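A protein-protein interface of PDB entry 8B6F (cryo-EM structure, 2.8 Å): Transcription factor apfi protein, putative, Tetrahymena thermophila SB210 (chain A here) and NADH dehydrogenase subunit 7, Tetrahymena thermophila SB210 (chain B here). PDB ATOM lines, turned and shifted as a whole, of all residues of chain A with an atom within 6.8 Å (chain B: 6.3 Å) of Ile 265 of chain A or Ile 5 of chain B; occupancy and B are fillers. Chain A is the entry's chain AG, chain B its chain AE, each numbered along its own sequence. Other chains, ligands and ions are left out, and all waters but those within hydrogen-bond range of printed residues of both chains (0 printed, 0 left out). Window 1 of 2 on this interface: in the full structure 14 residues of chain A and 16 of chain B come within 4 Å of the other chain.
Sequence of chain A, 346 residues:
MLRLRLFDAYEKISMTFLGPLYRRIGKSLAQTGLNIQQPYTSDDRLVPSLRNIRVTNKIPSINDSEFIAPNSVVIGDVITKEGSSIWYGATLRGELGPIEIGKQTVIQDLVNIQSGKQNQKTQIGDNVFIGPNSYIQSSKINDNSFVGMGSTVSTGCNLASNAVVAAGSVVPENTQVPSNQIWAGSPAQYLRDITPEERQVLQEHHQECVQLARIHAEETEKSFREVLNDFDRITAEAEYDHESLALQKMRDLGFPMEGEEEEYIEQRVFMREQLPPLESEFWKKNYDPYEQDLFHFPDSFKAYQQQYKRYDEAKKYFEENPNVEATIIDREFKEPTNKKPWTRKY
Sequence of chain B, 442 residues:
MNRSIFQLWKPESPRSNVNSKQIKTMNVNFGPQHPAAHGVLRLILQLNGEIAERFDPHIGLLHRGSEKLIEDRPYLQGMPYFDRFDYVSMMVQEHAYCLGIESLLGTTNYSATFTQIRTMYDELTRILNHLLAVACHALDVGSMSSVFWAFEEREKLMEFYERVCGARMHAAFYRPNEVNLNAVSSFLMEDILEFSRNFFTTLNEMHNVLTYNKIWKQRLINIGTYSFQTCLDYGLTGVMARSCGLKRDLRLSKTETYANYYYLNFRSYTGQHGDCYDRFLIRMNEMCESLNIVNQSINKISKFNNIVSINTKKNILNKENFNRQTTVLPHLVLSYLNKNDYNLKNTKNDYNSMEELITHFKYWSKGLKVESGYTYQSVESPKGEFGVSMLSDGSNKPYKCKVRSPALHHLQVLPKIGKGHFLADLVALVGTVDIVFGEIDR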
ATOM      1  N   LEU A 247       8.173 -12.073  17.332  1.00  0.00           N
ATOM      2  CA  LEU A 247       6.718 -11.993  17.397  1.00  0.00           C
ATOM      3  C   LEU A 247       6.121 -13.271  17.970  1.00  0.00           C
ATOM      4  O   LEU A 247       5.165 -13.219  18.751  1.00  0.00           O
ATOM      5  CB  LEU A 247       6.144 -11.711  16.010  1.00  0.00           C
ATOM      6  CG  LEU A 247       6.390 -10.319  15.431  1.00  0.00           C
ATOM      7  CD1 LEU A 247       5.953 -10.259  13.979  1.00  0.00           C
ATOM      8  CD2 LEU A 247       5.652  -9.275  16.252  1.00  0.00           C
ATOM      9  N   MET A 250       6.616 -13.100  21.632  1.00  0.00           N
ATOM     10  CA  MET A 250       5.754 -12.072  22.211  1.00  0.00           C
ATOM     11  C   MET A 250       4.310 -12.543  22.320  1.00  0.00           C
ATOM     12  O   MET A 250       3.652 -12.308  23.339  1.00  0.00           O
ATOM     13  CB  MET A 250       5.829 -10.796  21.376  1.00  0.00           C
ATOM     14  CG  MET A 250       7.140 -10.047  21.508  1.00  0.00           C
ATOM     15  SD  MET A 250       7.223  -8.623  20.413  1.00  0.00           S
ATOM     16  CE  MET A 250       8.918  -8.122  20.672  1.00  0.00           C
ATOM     17  N   PHE A 255       1.776 -10.433  24.536  1.00  0.00           N
ATOM     18  CA  PHE A 255       1.828  -9.035  24.148  1.00  0.00           C
ATOM     19  C   PHE A 255       0.735  -8.724  23.128  1.00  0.00           C
ATOM     20  O   PHE A 255       0.211  -9.625  22.470  1.00  0.00           O
ATOM     21  CB  PHE A 255       3.192  -8.691  23.555  1.00  0.00           C
ATOM     22  CG  PHE A 255       4.321  -8.702  24.552  1.00  0.00           C
ATOM     23  CD1 PHE A 255       4.135  -9.164  25.846  1.00  0.00           C
ATOM     24  CD2 PHE A 255       5.570  -8.228  24.192  1.00  0.00           C
ATOM     25  CE1 PHE A 255       5.176  -9.166  26.753  1.00  0.00           C
ATOM     26  CE2 PHE A 255       6.614  -8.228  25.092  1.00  0.00           C
ATOM     27  CZ  PHE A 255       6.417  -8.696  26.375  1.00  0.00           C
ATOM     28  N   PRO A 256       0.365  -7.452  22.987  1.00  0.00           N
ATOM     29  CA  PRO A 256      -0.604  -7.088  21.947  1.00  0.00           C
ATOM     30  C   PRO A 256      -0.076  -7.436  20.565  1.00  0.00           C
ATOM     31  O   PRO A 256       1.109  -7.265  20.274  1.00  0.00           O
ATOM     32  CB  PRO A 256      -0.766  -5.573  22.122  1.00  0.00           C
ATOM     33  CG  PRO A 256      -0.283  -5.284  23.500  1.00  0.00           C
ATOM     34  CD  PRO A 256       0.789  -6.284  23.777  1.00  0.00           C
ATOM     35  N   MET A 257      -0.976  -7.913  19.701  1.00  0.00           N
ATOM     36  CA  MET A 257      -0.623  -8.308  18.341  1.00  0.00           C
ATOM     37  C   MET A 257      -1.442  -7.562  17.293  1.00  0.00           C
ATOM     38  O   MET A 257      -1.473  -7.974  16.129  1.00  0.00           O
ATOM     39  CB  MET A 257      -0.799  -9.817  18.168  1.00  0.00           C
ATOM     40  CG  MET A 257       0.117 -10.668  19.043  1.00  0.00           C
ATOM     41  SD  MET A 257       1.799 -10.852  18.406  1.00  0.00           S
ATOM     42  CE  MET A 257       2.652  -9.472  19.161  1.00  0.00           C
ATOM     43  N   GLU A 261      -4.952  -2.918  19.748  1.00  0.00           N
ATOM     44  CA  GLU A 261      -4.518  -3.452  21.029  1.00  0.00           C
ATOM     45  C   GLU A 261      -3.186  -2.882  21.492  1.00  0.00           C
ATOM     46  O   GLU A 261      -2.793  -3.122  22.638  1.00  0.00           O
ATOM     47  CB  GLU A 261      -4.409  -4.978  20.952  1.00  0.00           C
ATOM     48  CG  GLU A 261      -5.728  -5.673  20.670  1.00  0.00           C
ATOM     49  CD  GLU A 261      -5.570  -7.167  20.493  1.00  0.00           C
ATOM     50  OE1 GLU A 261      -4.428  -7.622  20.281  1.00  0.00           O
ATOM     51  OE2 GLU A 261      -6.586  -7.886  20.568  1.00  0.00           O
ATOM     52  N   GLU A 262      -2.480  -2.141  20.634  1.00  0.00           N
ATOM     53  CA  GLU A 262      -1.217  -1.541  21.041  1.00  0.00           C
ATOM     54  C   GLU A 262      -1.392  -0.542  22.175  1.00  0.00           C
ATOM     55  O   GLU A 262      -0.416  -0.229  22.865  1.00  0.00           O
ATOM     56  CB  GLU A 262      -0.553  -0.841  19.853  1.00  0.00           C
ATOM     57  CG  GLU A 262      -0.081  -1.776  18.753  1.00  0.00           C
ATOM     58  CD  GLU A 262       0.976  -2.751  19.225  1.00  0.00           C
ATOM     59  OE1 GLU A 262       1.536  -2.535  20.319  1.00  0.00           O
ATOM     60  OE2 GLU A 262       1.243  -3.736  18.504  1.00  0.00           O
ATOM     61  N   GLU A 263      -2.605  -0.035  22.386  1.00  0.00           N
ATOM     62  CA  GLU A 263      -2.832   0.975  23.411  1.00  0.00           C
ATOM     63  C   GLU A 263      -2.947   0.390  24.812  1.00  0.00           C
ATOM     64  O   GLU A 263      -3.008   1.155  25.778  1.00  0.00           O
ATOM     65  CB  GLU A 263      -4.093   1.780  23.086  1.00  0.00           C
ATOM     66  CG  GLU A 263      -5.372   0.966  23.099  1.00  0.00           C
ATOM     67  CD  GLU A 263      -6.578   1.781  22.676  1.00  0.00           C
ATOM     68  OE1 GLU A 263      -6.455   3.021  22.592  1.00  0.00           O
ATOM     69  OE2 GLU A 263      -7.645   1.183  22.425  1.00  0.00           O
ATOM     70  N   TYR A 264      -2.984  -0.936  24.945  1.00  0.00           N
ATOM     71  CA  TYR A 264      -2.977  -1.603  26.240  1.00  0.00           C
ATOM     72  C   TYR A 264      -1.692  -2.396  26.449  1.00  0.00           C
ATOM     73  O   TYR A 264      -1.688  -3.420  27.134  1.00  0.00           O
ATOM     74  CB  TYR A 264      -4.196  -2.516  26.374  1.00  0.00           C
ATOM     75  CG  TYR A 264      -5.508  -1.770  26.323  1.00  0.00           C
ATOM     76  CD1 TYR A 264      -5.983  -1.082  27.431  1.00  0.00           C
ATOM     77  CD2 TYR A 264      -6.273  -1.757  25.165  1.00  0.00           C
ATOM     78  CE1 TYR A 264      -7.180  -0.397  27.388  1.00  0.00           C
ATOM     79  CE2 TYR A 264      -7.473  -1.076  25.111  1.00  0.00           C
ATOM     80  CZ  TYR A 264      -7.922  -0.398  26.225  1.00  0.00           C
ATOM     81  OH  TYR A 264      -9.116   0.281  26.176  1.00  0.00           O
ATOM     82  N   ILE A 265      -0.593  -1.930  25.853  1.00  0.00           N
ATOM     83  CA  ILE A 265       0.677  -2.643  25.964  1.00  0.00           C
ATOM     84  C   ILE A 265       1.154  -2.672  27.409  1.00  0.00           C
ATOM     85  O   ILE A 265       1.632  -3.703  27.897  1.00  0.00           O
ATOM     86  CB  ILE A 265       1.724  -2.009  25.027  1.00  0.00           C
ATOM     87  CG1 ILE A 265       3.031  -2.808  25.079  1.00  0.00           C
ATOM     88  CG2 ILE A 265       1.962  -0.540  25.389  1.00  0.00           C
ATOM     89  CD1 ILE A 265       4.102  -2.314  24.124  1.00  0.00           C
ATOM     90  N   GLU A 266       1.038  -1.547  28.119  1.00  0.00           N
ATOM     91  CA  GLU A 266       1.579  -1.476  29.472  1.00  0.00           C
ATOM     92  C   GLU A 266       0.940  -2.505  30.393  1.00  0.00           C
ATOM     93  O   GLU A 266       1.578  -2.965  31.345  1.00  0.00           O
ATOM     94  CB  GLU A 266       1.399  -0.067  30.047  1.00  0.00           C
ATOM     95  CG  GLU A 266      -0.045   0.366  30.297  1.00  0.00           C
ATOM     96  CD  GLU A 266      -0.768   0.779  29.033  1.00  0.00           C
ATOM     97  OE1 GLU A 266      -0.147   0.737  27.951  1.00  0.00           O
ATOM     98  OE2 GLU A 266      -1.958   1.150  29.120  1.00  0.00           O
ATOM     99  N   GLN A 267      -0.312  -2.883  30.128  1.00  0.00           N
ATOM    100  CA  GLN A 267      -0.981  -3.875  30.959  1.00  0.00           C
ATOM    101  C   GLN A 267      -0.413  -5.275  30.783  1.00  0.00           C
ATOM    102  O   GLN A 267      -0.689  -6.147  31.611  1.00  0.00           O
ATOM    103  CB  GLN A 267      -2.475  -3.899  30.648  1.00  0.00           C
ATOM    104  CG  GLN A 267      -3.301  -3.010  31.544  1.00  0.00           C
ATOM    105  CD  GLN A 267      -2.993  -1.543  31.369  1.00  0.00           C
ATOM    106  OE1 GLN A 267      -2.830  -1.061  30.250  1.00  0.00           O
ATOM    107  NE2 GLN A 267      -2.909  -0.821  32.479  1.00  0.00           N
ATOM    108  N   ARG A 268       0.367  -5.512  29.730  1.00  0.00           N
ATOM    109  CA  ARG A 268       0.889  -6.838  29.441  1.00  0.00           C
ATOM    110  C   ARG A 268       2.401  -6.945  29.533  1.00  0.00           C
ATOM    111  O   ARG A 268       2.915  -8.067  29.591  1.00  0.00           O
ATOM    112  CB  ARG A 268       0.458  -7.286  28.034  1.00  0.00           C
ATOM    113  CG  ARG A 268      -0.899  -7.970  27.990  1.00  0.00           C
ATOM    114  CD  ARG A 268      -0.855  -9.332  28.664  1.00  0.00           C
ATOM    115  NE  ARG A 268      -1.982 -10.169  28.275  1.00  0.00           N
ATOM    116  CZ  ARG A 268      -3.152 -10.202  28.900  1.00  0.00           C
ATOM    117  NH1 ARG A 268      -3.391  -9.450  29.962  1.00  0.00           N
ATOM    118  NH2 ARG A 268      -4.106 -11.009  28.446  1.00  0.00           N
ATOM    119  N   VAL A 269       3.123  -5.829  29.553  1.00  0.00           N
ATOM    120  CA  VAL A 269       4.577  -5.839  29.564  1.00  0.00           C
ATOM    121  C   VAL A 269       5.131  -5.355  30.898  1.00  0.00           C
ATOM    122  O   VAL A 269       6.124  -5.898  31.390  1.00  0.00           O
ATOM    123  CB  VAL A 269       5.140  -4.998  28.394  1.00  0.00           C
ATOM    124  CG1 VAL A 269       4.559  -5.469  27.073  1.00  0.00           C
ATOM    125  CG2 VAL A 269       4.869  -3.514  28.597  1.00  0.00           C
ATOM    126  N   PHE A 270       4.506  -4.349  31.501  1.00  0.00           N
ATOM    127  CA  PHE A 270       5.044  -3.696  32.687  1.00  0.00           C
ATOM    128  C   PHE A 270       4.156  -3.824  33.912  1.00  0.00           C
ATOM    129  O   PHE A 270       4.669  -4.002  35.019  1.00  0.00           O
ATOM    130  CB  PHE A 270       5.287  -2.209  32.387  1.00  0.00           C
ATOM    131  CG  PHE A 270       5.867  -1.445  33.540  1.00  0.00           C
ATOM    132  CD1 PHE A 270       7.024  -1.880  34.164  1.00  0.00           C
ATOM    133  CD2 PHE A 270       5.268  -0.280  33.985  1.00  0.00           C
ATOM    134  CE1 PHE A 270       7.563  -1.177  35.220  1.00  0.00           C
ATOM    135  CE2 PHE A 270       5.803   0.427  35.040  1.00  0.00           C
ATOM    136  CZ  PHE A 270       6.951  -0.021  35.659  1.00  0.00           C
ATOM    137  N   MET A 271       2.834  -3.742  33.750  1.00  0.00           N
ATOM    138  CA  MET A 271       1.951  -3.739  34.912  1.00  0.00           C
ATOM    139  C   MET A 271       2.035  -5.049  35.686  1.00  0.00           C
ATOM    140  O   MET A 271       2.031  -5.044  36.923  1.00  0.00           O
ATOM    141  CB  MET A 271       0.512  -3.471  34.472  1.00  0.00           C
ATOM    142  CG  MET A 271       0.246  -2.021  34.091  1.00  0.00           C
ATOM    143  SD  MET A 271       0.415  -0.891  35.484  1.00  0.00           S
ATOM    144  CE  MET A 271       0.056   0.674  34.696  1.00  0.00           C
ATOM    145  N   ARG B   3       1.021  -3.744  13.249  1.00  0.00           N
ATOM    146  CA  ARG B   3       1.701  -3.852  14.531  1.00  0.00           C
ATOM    147  C   ARG B   3       2.745  -2.753  14.685  1.00  0.00           C
ATOM    148  O   ARG B   3       3.321  -2.267  13.708  1.00  0.00           O
ATOM    149  CB  ARG B   3       2.378  -5.214  14.675  1.00  0.00           C
ATOM    150  CG  ARG B   3       1.479  -6.404  14.400  1.00  0.00           C
ATOM    151  CD  ARG B   3       2.150  -7.686  14.863  1.00  0.00           C
ATOM    152  NE  ARG B   3       1.517  -8.879  14.314  1.00  0.00           N
ATOM    153  CZ  ARG B   3       1.873  -9.469  13.181  1.00  0.00           C
ATOM    154  NH1 ARG B   3       2.853  -8.994  12.430  1.00  0.00           N
ATOM    155  NH2 ARG B   3       1.232 -10.568  12.793  1.00  0.00           N
ATOM    156  N   SER B   4       2.979  -2.356  15.939  1.00  0.00           N
ATOM    157  CA  SER B   4       4.028  -1.392  16.250  1.00  0.00           C
ATOM    158  C   SER B   4       4.776  -1.762  17.527  1.00  0.00           C
ATOM    159  O   SER B   4       5.392  -0.889  18.147  1.00  0.00           O
ATOM    160  CB  SER B   4       3.449   0.018  16.393  1.00  0.00           C
ATOM    161  OG  SER B   4       2.831   0.441  15.190  1.00  0.00           O
ATOM    162  N   ILE B   5       4.748  -3.034  17.927  1.00  0.00           N
ATOM    163  CA  ILE B   5       5.357  -3.428  19.195  1.00  0.00           C
ATOM    164  C   ILE B   5       6.851  -3.132  19.184  1.00  0.00           C
ATOM    165  O   ILE B   5       7.403  -2.613  20.162  1.00  0.00           O
ATOM    166  CB  ILE B   5       5.065  -4.912  19.488  1.00  0.00           C
ATOM    167  CG1 ILE B   5       5.642  -5.328  20.847  1.00  0.00           C
ATOM    168  CG2 ILE B   5       5.617  -5.809  18.389  1.00  0.00           C
ATOM    169  CD1 ILE B   5       5.024  -4.613  22.029  1.00  0.00           C
ATOM    170  N   PHE B   6       7.530  -3.447  18.079  1.00  0.00           N
ATOM    171  CA  PHE B   6       8.970  -3.230  18.011  1.00  0.00           C
ATOM    172  C   PHE B   6       9.319  -1.749  18.044  1.00  0.00           C
ATOM    173  O   PHE B   6      10.362  -1.371  18.589  1.00  0.00           O
ATOM    174  CB  PHE B   6       9.541  -3.886  16.758  1.00  0.00           C
ATOM    175  CG  PHE B   6       9.324  -5.367  16.707  1.00  0.00           C
ATOM    176  CD1 PHE B   6      10.022  -6.211  17.553  1.00  0.00           C
ATOM    177  CD2 PHE B   6       8.429  -5.917  15.807  1.00  0.00           C
ATOM    178  CE1 PHE B   6       9.824  -7.576  17.507  1.00  0.00           C
ATOM    179  CE2 PHE B   6       8.230  -7.279  15.757  1.00  0.00           C
ATOM    180  CZ  PHE B   6       8.930  -8.111  16.607  1.00  0.00           C
ATOM    181  N   GLN B   7       8.475  -0.901  17.463  1.00  0.00           N
ATOM    182  CA  GLN B   7       8.680   0.537  17.554  1.00  0.00           C
ATOM    183  C   GLN B   7       8.280   1.094  18.912  1.00  0.00           C
ATOM    184  O   GLN B   7       8.667   2.220  19.242  1.00  0.00           O
ATOM    185  CB  GLN B   7       7.884   1.253  16.461  1.00  0.00           C
ATOM    186  CG  GLN B   7       8.175   0.759  15.058  1.00  0.00           C
ATOM    187  CD  GLN B   7       7.374   1.499  14.009  1.00  0.00           C
ATOM    188  OE1 GLN B   7       6.938   2.628  14.226  1.00  0.00           O
ATOM    189  NE2 GLN B   7       7.170   0.860  12.862  1.00  0.00           N
ATOM    190  N   LEU B   8       7.524   0.335  19.705  1.00  0.00           N
ATOM    191  CA  LEU B   8       7.013   0.823  20.978  1.00  0.00           C
ATOM    192  C   LEU B   8       7.832   0.390  22.186  1.00  0.00           C
ATOM    193  O   LEU B   8       7.743   1.043  23.229  1.00  0.00           O
ATOM    194  CB  LEU B   8       5.565   0.359  21.172  1.00  0.00           C
ATOM    195  CG  LEU B   8       4.511   1.066  20.317  1.00  0.00           C
ATOM    196  CD1 LEU B   8       3.171   0.372  20.462  1.00  0.00           C
ATOM    197  CD2 LEU B   8       4.396   2.534  20.689  1.00  0.00           C
ATOM    198  N   TRP B   9       8.612  -0.686  22.089  1.00  0.00           N
ATOM    199  CA  TRP B   9       9.421  -1.138  23.211  1.00  0.00           C
ATOM    200  C   TRP B   9      10.821  -1.492  22.730  1.00  0.00           C
ATOM    201  O   TRP B   9      11.015  -1.918  21.589  1.00  0.00           O
ATOM    202  CB  TRP B   9       8.762  -2.334  23.919  1.00  0.00           C
ATOM    203  CG  TRP B   9       9.226  -3.689  23.470  1.00  0.00           C
ATOM    204  CD1 TRP B   9       9.285  -4.158  22.191  1.00  0.00           C
ATOM    205  CD2 TRP B   9       9.672  -4.759  24.310  1.00  0.00           C
ATOM    206  NE1 TRP B   9       9.749  -5.449  22.182  1.00  0.00           N
ATOM    207  CE2 TRP B   9       9.996  -5.841  23.471  1.00  0.00           C
ATOM    208  CE3 TRP B   9       9.836  -4.904  25.692  1.00  0.00           C
ATOM    209  CZ2 TRP B   9      10.475  -7.052  23.966  1.00  0.00           C
ATOM    210  CZ3 TRP B   9      10.312  -6.107  26.182  1.00  0.00           C
ATOM    211  CH2 TRP B   9      10.626  -7.166  25.320  1.00  0.00           C
ATOM    212  N   LYS B  10      11.798  -1.299  23.615  1.00  0.00           N
ATOM    213  CA  LYS B  10      13.199  -1.597  23.319  1.00  0.00           C
ATOM    214  C   LYS B  10      13.804  -2.331  24.511  1.00  0.00           C
ATOM    215  O   LYS B  10      14.192  -1.694  25.503  1.00  0.00           O
ATOM    216  CB  LYS B  10      13.986  -0.326  23.013  1.00  0.00           C
ATOM    217  CG  LYS B  10      15.479  -0.562  22.849  1.00  0.00           C
ATOM    218  CD  LYS B  10      16.208   0.698  22.425  1.00  0.00           C
ATOM    219  CE  LYS B  10      17.707   0.453  22.345  1.00  0.00           C
ATOM    220  NZ  LYS B  10      18.464   1.680  21.974  1.00  0.00           N
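The backbone carbonyl oxygen (O) of Met 250 of chain A lies within hydrogen-bond range of the backbone NH (N) of Phe 255 of chain A, at 2.9 Å.
Hydrophobic or aromatic side chains of chain B that line the printed part of chain A: Ile 5, Phe 6, Leu 8 and Trp 9. Printed residues of chain A that touch a printed residue of chain B: Leu 247, Met 250, Met 257, Glu 262 and Ile 265. Among the printed residues, no Asp or Glu carboxylate lies within 4 Å of a Lys or Arg side-chain nitrogen of the other chain.
Among the printed residues, pairs that only touch across the chains: Leu 247 of chain A with Arg 3 of chain B, Leu 247 of chain A with Phe 6 of chain B, Met 250 of chain A with Ile 5 of chain B, Met 250 of chain A with Phe 6 of chain B, Met 250 of chain A with Trp 9 of chain B, Met 257 of chain A with Arg 3 of chain B, Glu 262 of chain A with Ile 5 of chain B, Glu 262 of chain A with Leu 8 of chain B and Ile 265 of chain A with Ile 5 of chain B.
Of chain B, only Ile 5 (3.2 Å) comes within 4 Å of Ile 265 of chain A. Of chain A, only Met 250, Glu 262 and Ile 265 come within 4 Å of Ile 5 of chain B. Printed residues of chain A within 4 Å of Arg 3 of chain B: Leu 247 (3.7 Å) and Met 257 (3.6 Å). Printed residues of chain A within 4 Å of Trp 9 of chain B: Met 250. Printed residues of chain B within 4 Å of Met 257 of chain A: Arg 3. The nearest residue of chain A that does not touch Ile 5 of chain B is Leu 247 of chain A (4.1 Å). The nearest printed residue of chain B that does not touch Met 257 of chain A is Ile 5 of chain B (4.8 Å).
The side-chain carboxylate (OE2) of Glu 262 of chain A lies within hydrogen-bond range of the backbone NH (N) of Ser 4 of chain B.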
